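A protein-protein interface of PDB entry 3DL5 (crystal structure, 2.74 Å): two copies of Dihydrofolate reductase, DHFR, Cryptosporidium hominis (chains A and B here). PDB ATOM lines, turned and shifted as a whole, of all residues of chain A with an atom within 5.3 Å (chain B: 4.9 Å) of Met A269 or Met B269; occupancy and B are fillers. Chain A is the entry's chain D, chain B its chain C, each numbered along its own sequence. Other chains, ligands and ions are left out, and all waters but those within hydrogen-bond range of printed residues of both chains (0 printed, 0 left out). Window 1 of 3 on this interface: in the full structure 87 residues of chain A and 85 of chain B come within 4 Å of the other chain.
The guanidinium group (NH2) of Arg A271 sits close to the backbone carbonyl oxygen (O) of Gly B267 (2.3 Å).
The guanidinium group (NH2) of Arg B271 is in hydrogen-bond range of the backbone carbonyl oxygen (O) of Gly A267 (2.5 Å).
NE2 of Gln B268 lies close to NH2 of Arg A271 (2.8 Å).
The side-chain amide nitrogen (NE2) of Gln A268 lies close to the guanidinium group (NH2) of Arg B271 (3.3 Å).
The side-chain amide oxygen of Gln B239 lies within hydrogen-bond range of the backbone NH of Arg B271 (3.3 Å).
The side-chain amide oxygen of Gln A268 lies within hydrogen-bond range of the guanidinium group of Arg A246 (2.7 Å).
The backbone NH (N) of Gly A267 sits close to the backbone carbonyl oxygen (O) of Ile A460 (3.3 Å).
NH1 of Arg B246 lies within hydrogen-bond range of OE1 of Gln B268 (2.4 Å).
The side-chain amide oxygen of Gln A239 sits at hydrogen-bond distance from the backbone NH of Arg A271 (2.9 Å).
N of Gln B268 is in hydrogen-bond range of O of Ile B460.
CZ of Phe B459 touches O of Gln A268 (3.99 Å).
Met B269 touches Met A269 (CE to CE, 3.2 Å).
CE2 of Phe A459 touches O of Gln B268, at 3.7 Å.
Phe B459 touches Phe A459 (CD2 to CD2, 3.1 Å).
Met A269 touches just one residue of chain B: Met B269.
Of the printed residues of chain B, Gly A267 touches Arg B271.
Of the printed residues of chain A, Phe B459 touches Gln A268 (3.99 Å) and Phe A459 (3.1 Å).
Of the printed residues of chain A, Gly B267 touches Arg A271 (2.3 Å).
Of the printed residues of chain B, Gln A268 touches Arg B271 and Phe B459.
The nearest residue of chain B that does not touch Met A269 is Phe B459 (4.6 Å).
The nearest residue of chain A that does not touch Met B269 is Phe A459 (4.8 Å).
Of the 10 printed residues of chain B, 5 touch a printed residue of chain A.
Hydrophobic or aromatic side chains of chain B within 4 Å of the printed part of chain A: Met B269 and Phe B459.
Among the printed residues, 8 pairs touch across the chains.
Gly A267 touches Arg B271, and with the chains exchanged Arg A271 touches Gly B267.
Gln A268 touches Phe B459, and with the chains exchanged Phe A459 touches Gln B268.
Met B269 touches its own counterpart, Met A269.
Phe A459 touches its own counterpart, Phe B459.
Of the 8 pairs that touch across the chains among the printed residues, 8 have their exchanged pair printed and touching as well.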
ATOM      1  N   GLN A 239      -8.645 -29.480 -10.330  1.00  0.00           N
ATOM      2  CA  GLN A 239      -7.656 -28.683 -11.046  1.00  0.00           C
ATOM      3  C   GLN A 239      -6.407 -29.502 -11.355  1.00  0.00           C
ATOM      4  O   GLN A 239      -5.835 -29.395 -12.440  1.00  0.00           O
ATOM      5  CB  GLN A 239      -7.281 -27.440 -10.236  1.00  0.00           C
ATOM      6  CG  GLN A 239      -8.424 -26.456 -10.047  1.00  0.00           C
ATOM      7  CD  GLN A 239      -8.678 -25.611 -11.280  1.00  0.00           C
ATOM      8  OE1 GLN A 239      -7.744 -25.103 -11.901  1.00  0.00           O
ATOM      9  NE2 GLN A 239      -9.946 -25.458 -11.641  1.00  0.00           N
ATOM     10  N   ARG A 246      -5.708 -34.608 -18.752  1.00  0.00           N
ATOM     11  CA  ARG A 246      -5.576 -33.811 -19.958  1.00  0.00           C
ATOM     12  C   ARG A 246      -4.259 -34.164 -20.674  1.00  0.00           C
ATOM     13  O   ARG A 246      -4.190 -34.124 -21.904  1.00  0.00           O
ATOM     14  CB  ARG A 246      -5.629 -32.329 -19.607  1.00  0.00           C
ATOM     15  CG  ARG A 246      -6.278 -31.454 -20.659  1.00  0.00           C
ATOM     16  CD  ARG A 246      -6.380 -30.014 -20.169  1.00  0.00           C
ATOM     17  NE  ARG A 246      -7.284 -29.886 -19.030  1.00  0.00           N
ATOM     18  CZ  ARG A 246      -6.962 -29.325 -17.867  1.00  0.00           C
ATOM     19  NH1 ARG A 246      -5.748 -28.829 -17.662  1.00  0.00           N
ATOM     20  NH2 ARG A 246      -7.868 -29.256 -16.904  1.00  0.00           N
ATOM     21  N   GLY A 267       2.206 -25.614 -21.436  1.00  0.00           N
ATOM     22  CA  GLY A 267       1.341 -24.509 -21.048  1.00  0.00           C
ATOM     23  C   GLY A 267      -0.002 -24.843 -20.418  1.00  0.00           C
ATOM     24  O   GLY A 267      -1.031 -24.841 -21.082  1.00  0.00           O
ATOM     25  N   GLN A 268       0.004 -25.116 -19.122  1.00  0.00           N
ATOM     26  CA  GLN A 268      -1.221 -25.439 -18.404  1.00  0.00           C
ATOM     27  C   GLN A 268      -1.294 -24.609 -17.122  1.00  0.00           C
ATOM     28  O   GLN A 268      -0.335 -23.930 -16.766  1.00  0.00           O
ATOM     29  CB  GLN A 268      -1.248 -26.936 -18.082  1.00  0.00           C
ATOM     30  CG  GLN A 268      -1.420 -27.812 -19.310  1.00  0.00           C
ATOM     31  CD  GLN A 268      -2.776 -27.619 -19.965  1.00  0.00           C
ATOM     32  OE1 GLN A 268      -3.800 -28.015 -19.418  1.00  0.00           O
ATOM     33  NE2 GLN A 268      -2.789 -26.997 -21.136  1.00  0.00           N
ATOM     34  N   MET A 269      -2.434 -24.645 -16.441  1.00  0.00           N
ATOM     35  CA  MET A 269      -2.594 -23.892 -15.200  1.00  0.00           C
ATOM     36  C   MET A 269      -3.574 -24.554 -14.229  1.00  0.00           C
ATOM     37  O   MET A 269      -4.471 -25.297 -14.642  1.00  0.00           O
ATOM     38  CB  MET A 269      -3.076 -22.468 -15.492  1.00  0.00           C
ATOM     39  CG  MET A 269      -4.579 -22.323 -15.620  1.00  0.00           C
ATOM     40  SD  MET A 269      -5.094 -20.656 -15.108  1.00  0.00           S
ATOM     41  CE  MET A 269      -6.484 -20.351 -16.264  1.00  0.00           C
ATOM     42  N   MET A 270      -3.386 -24.272 -12.938  1.00  0.00           N
ATOM     43  CA  MET A 270      -4.237 -24.799 -11.872  1.00  0.00           C
ATOM     44  C   MET A 270      -4.501 -23.716 -10.840  1.00  0.00           C
ATOM     45  O   MET A 270      -3.611 -22.936 -10.521  1.00  0.00           O
ATOM     46  CB  MET A 270      -3.566 -25.976 -11.163  1.00  0.00           C
ATOM     47  CG  MET A 270      -3.236 -27.169 -12.039  1.00  0.00           C
ATOM     48  SD  MET A 270      -2.518 -28.527 -11.065  1.00  0.00           S
ATOM     49  CE  MET A 270      -0.818 -27.970 -10.882  1.00  0.00           C
ATOM     50  N   ARG A 271      -5.726 -23.668 -10.324  1.00  0.00           N
ATOM     51  CA  ARG A 271      -6.109 -22.701  -9.294  1.00  0.00           C
ATOM     52  C   ARG A 271      -6.422 -23.449  -8.015  1.00  0.00           C
ATOM     53  O   ARG A 271      -6.841 -24.601  -8.053  1.00  0.00           O
ATOM     54  CB  ARG A 271      -7.367 -21.940  -9.675  1.00  0.00           C
ATOM     55  CG  ARG A 271      -7.203 -20.877 -10.708  1.00  0.00           C
ATOM     56  CD  ARG A 271      -8.374 -19.919 -10.630  1.00  0.00           C
ATOM     57  NE  ARG A 271      -7.936 -18.573 -10.963  1.00  0.00           N
ATOM     58  CZ  ARG A 271      -7.782 -18.133 -12.203  1.00  0.00           C
ATOM     59  NH1 ARG A 271      -8.046 -18.927 -13.234  1.00  0.00           N
ATOM     60  NH2 ARG A 271      -7.336 -16.910 -12.411  1.00  0.00           N
ATOM     61  N   ILE A 458      -0.952 -22.002 -10.284  1.00  0.00           N
ATOM     62  CA  ILE A 458       0.289 -22.542 -10.811  1.00  0.00           C
ATOM     63  C   ILE A 458       0.231 -22.625 -12.333  1.00  0.00           C
ATOM     64  O   ILE A 458      -0.664 -23.251 -12.905  1.00  0.00           O
ATOM     65  CB  ILE A 458       0.579 -23.925 -10.220  1.00  0.00           C
ATOM     66  CG1 ILE A 458       0.735 -23.792  -8.701  1.00  0.00           C
ATOM     67  CG2 ILE A 458       1.835 -24.508 -10.840  1.00  0.00           C
ATOM     68  CD1 ILE A 458       0.887 -25.106  -7.968  1.00  0.00           C
ATOM     69  N   PHE A 459       1.174 -21.946 -12.982  1.00  0.00           N
ATOM     70  CA  PHE A 459       1.259 -21.938 -14.434  1.00  0.00           C
ATOM     71  C   PHE A 459       2.404 -22.857 -14.821  1.00  0.00           C
ATOM     72  O   PHE A 459       3.528 -22.710 -14.333  1.00  0.00           O
ATOM     73  CB  PHE A 459       1.515 -20.529 -14.932  1.00  0.00           C
ATOM     74  CG  PHE A 459       0.497 -19.532 -14.464  1.00  0.00           C
ATOM     75  CD1 PHE A 459       0.829 -18.578 -13.516  1.00  0.00           C
ATOM     76  CD2 PHE A 459      -0.789 -19.526 -14.992  1.00  0.00           C
ATOM     77  CE1 PHE A 459      -0.103 -17.623 -13.100  1.00  0.00           C
ATOM     78  CE2 PHE A 459      -1.730 -18.577 -14.586  1.00  0.00           C
ATOM     79  CZ  PHE A 459      -1.382 -17.620 -13.635  1.00  0.00           C
ATOM     80  N   ILE A 460       2.117 -23.808 -15.699  1.00  0.00           N
ATOM     81  CA  ILE A 460       3.118 -24.779 -16.097  1.00  0.00           C
ATOM     82  C   ILE A 460       3.584 -24.733 -17.541  1.00  0.00           C
ATOM     83  O   ILE A 460       2.823 -24.422 -18.459  1.00  0.00           O
ATOM     84  CB  ILE A 460       2.612 -26.200 -15.788  1.00  0.00           C
ATOM     85  CG1 ILE A 460       2.187 -26.273 -14.316  1.00  0.00           C
ATOM     86  CG2 ILE A 460       3.703 -27.229 -16.087  1.00  0.00           C
ATOM     87  CD1 ILE A 460       1.580 -27.612 -13.902  1.00  0.00           C
ATOM     88  N   GLN B 239     -10.048 -14.676 -26.091  1.00  0.00           N
ATOM     89  CA  GLN B 239      -9.198 -14.955 -24.942  1.00  0.00           C
ATOM     90  C   GLN B 239      -8.795 -13.628 -24.337  1.00  0.00           C
ATOM     91  O   GLN B 239      -8.557 -13.533 -23.131  1.00  0.00           O
ATOM     92  CB  GLN B 239      -7.934 -15.692 -25.354  1.00  0.00           C
ATOM     93  CG  GLN B 239      -8.175 -17.047 -25.934  1.00  0.00           C
ATOM     94  CD  GLN B 239      -8.478 -18.070 -24.887  1.00  0.00           C
ATOM     95  OE1 GLN B 239      -7.759 -18.188 -23.896  1.00  0.00           O
ATOM     96  NE2 GLN B 239      -9.530 -18.837 -25.103  1.00  0.00           N
ATOM     97  N   ARG B 246     -13.802 -10.031 -17.697  1.00  0.00           N
ATOM     98  CA  ARG B 246     -13.578 -10.595 -16.387  1.00  0.00           C
ATOM     99  C   ARG B 246     -13.102  -9.561 -15.382  1.00  0.00           C
ATOM    100  O   ARG B 246     -13.519  -9.601 -14.221  1.00  0.00           O
ATOM    101  CB  ARG B 246     -12.580 -11.743 -16.486  1.00  0.00           C
ATOM    102  CG  ARG B 246     -13.192 -13.110 -16.243  1.00  0.00           C
ATOM    103  CD  ARG B 246     -12.176 -14.195 -16.492  1.00  0.00           C
ATOM    104  NE  ARG B 246     -12.046 -14.451 -17.919  1.00  0.00           N
ATOM    105  CZ  ARG B 246     -10.910 -14.758 -18.535  1.00  0.00           C
ATOM    106  NH1 ARG B 246      -9.770 -14.849 -17.861  1.00  0.00           N
ATOM    107  NH2 ARG B 246     -10.924 -14.980 -19.839  1.00  0.00           N
ATOM    108  N   GLY B 267      -3.730 -13.213 -11.567  1.00  0.00           N
ATOM    109  CA  GLY B 267      -3.599 -14.561 -12.105  1.00  0.00           C
ATOM    110  C   GLY B 267      -4.558 -14.990 -13.210  1.00  0.00           C
ATOM    111  O   GLY B 267      -5.499 -15.728 -12.957  1.00  0.00           O
ATOM    112  N   GLN B 268      -4.336 -14.531 -14.438  1.00  0.00           N
ATOM    113  CA  GLN B 268      -5.192 -14.913 -15.561  1.00  0.00           C
ATOM    114  C   GLN B 268      -4.370 -15.592 -16.653  1.00  0.00           C
ATOM    115  O   GLN B 268      -3.151 -15.723 -16.532  1.00  0.00           O
ATOM    116  CB  GLN B 268      -5.924 -13.695 -16.139  1.00  0.00           C
ATOM    117  CG  GLN B 268      -6.929 -13.102 -15.185  1.00  0.00           C
ATOM    118  CD  GLN B 268      -8.010 -14.092 -14.801  1.00  0.00           C
ATOM    119  OE1 GLN B 268      -8.805 -14.520 -15.635  1.00  0.00           O
ATOM    120  NE2 GLN B 268      -8.044 -14.461 -13.530  1.00  0.00           N
ATOM    121  N   MET B 269      -5.043 -16.008 -17.725  1.00  0.00           N
ATOM    122  CA  MET B 269      -4.387 -16.703 -18.825  1.00  0.00           C
ATOM    123  C   MET B 269      -5.030 -16.427 -20.189  1.00  0.00           C
ATOM    124  O   MET B 269      -6.210 -16.077 -20.268  1.00  0.00           O
ATOM    125  CB  MET B 269      -4.405 -18.198 -18.522  1.00  0.00           C
ATOM    126  CG  MET B 269      -4.271 -19.079 -19.716  1.00  0.00           C
ATOM    127  SD  MET B 269      -4.169 -20.800 -19.233  1.00  0.00           S
ATOM    128  CE  MET B 269      -5.896 -21.271 -19.248  1.00  0.00           C
ATOM    129  N   MET B 270      -4.237 -16.577 -21.254  1.00  0.00           N
ATOM    130  CA  MET B 270      -4.681 -16.383 -22.644  1.00  0.00           C
ATOM    131  C   MET B 270      -3.881 -17.296 -23.583  1.00  0.00           C
ATOM    132  O   MET B 270      -2.655 -17.355 -23.498  1.00  0.00           O
ATOM    133  CB  MET B 270      -4.462 -14.938 -23.107  1.00  0.00           C
ATOM    134  CG  MET B 270      -5.345 -13.881 -22.478  1.00  0.00           C
ATOM    135  SD  MET B 270      -5.172 -12.258 -23.304  1.00  0.00           S
ATOM    136  CE  MET B 270      -3.559 -11.738 -22.755  1.00  0.00           C
ATOM    137  N   ARG B 271      -4.563 -18.008 -24.473  1.00  0.00           N
ATOM    138  CA  ARG B 271      -3.867 -18.866 -25.430  1.00  0.00           C
ATOM    139  C   ARG B 271      -4.169 -18.319 -26.806  1.00  0.00           C
ATOM    140  O   ARG B 271      -5.225 -17.742 -27.030  1.00  0.00           O
ATOM    141  CB  ARG B 271      -4.362 -20.311 -25.403  1.00  0.00           C
ATOM    142  CG  ARG B 271      -4.659 -20.873 -24.051  1.00  0.00           C
ATOM    143  CD  ARG B 271      -4.959 -22.356 -24.170  1.00  0.00           C
ATOM    144  NE  ARG B 271      -3.728 -23.135 -24.171  1.00  0.00           N
ATOM    145  CZ  ARG B 271      -3.349 -23.917 -23.165  1.00  0.00           C
ATOM    146  NH1 ARG B 271      -4.108 -24.026 -22.083  1.00  0.00           N
ATOM    147  NH2 ARG B 271      -2.210 -24.590 -23.245  1.00  0.00           N
ATOM    148  N   ILE B 458      -0.079 -16.915 -22.624  1.00  0.00           N
ATOM    149  CA  ILE B 458       0.377 -15.840 -21.748  1.00  0.00           C
ATOM    150  C   ILE B 458      -0.277 -15.920 -20.376  1.00  0.00           C
ATOM    151  O   ILE B 458      -1.502 -15.913 -20.254  1.00  0.00           O
ATOM    152  CB  ILE B 458       0.081 -14.463 -22.374  1.00  0.00           C
ATOM    153  CG1 ILE B 458       0.909 -14.293 -23.650  1.00  0.00           C
ATOM    154  CG2 ILE B 458       0.390 -13.364 -21.388  1.00  0.00           C
ATOM    155  CD1 ILE B 458       0.659 -12.988 -24.386  1.00  0.00           C
ATOM    156  N   PHE B 459       0.558 -16.010 -19.348  1.00  0.00           N
ATOM    157  CA  PHE B 459       0.096 -16.093 -17.966  1.00  0.00           C
ATOM    158  C   PHE B 459       0.318 -14.748 -17.313  1.00  0.00           C
ATOM    159  O   PHE B 459       1.434 -14.255 -17.257  1.00  0.00           O
ATOM    160  CB  PHE B 459       0.857 -17.189 -17.239  1.00  0.00           C
ATOM    161  CG  PHE B 459       0.784 -18.512 -17.934  1.00  0.00           C
ATOM    162  CD1 PHE B 459       1.910 -19.071 -18.511  1.00  0.00           C
ATOM    163  CD2 PHE B 459      -0.426 -19.193 -18.030  1.00  0.00           C
ATOM    164  CE1 PHE B 459       1.834 -20.295 -19.174  1.00  0.00           C
ATOM    165  CE2 PHE B 459      -0.514 -20.409 -18.684  1.00  0.00           C
ATOM    166  CZ  PHE B 459       0.618 -20.964 -19.259  1.00  0.00           C
ATOM    167  N   ILE B 460      -0.761 -14.161 -16.812  1.00  0.00           N
ATOM    168  CA  ILE B 460      -0.702 -12.844 -16.216  1.00  0.00           C
ATOM    169  C   ILE B 460      -0.870 -12.795 -14.712  1.00  0.00           C
ATOM    170  O   ILE B 460      -1.695 -13.506 -14.142  1.00  0.00           O
ATOM    171  CB  ILE B 460      -1.768 -11.946 -16.848  1.00  0.00           C
ATOM    172  CG1 ILE B 460      -1.536 -11.885 -18.357  1.00  0.00           C
ATOM    173  CG2 ILE B 460      -1.730 -10.560 -16.224  1.00  0.00           C
ATOM    174  CD1 ILE B 460      -2.591 -11.110 -19.127  1.00  0.00           C
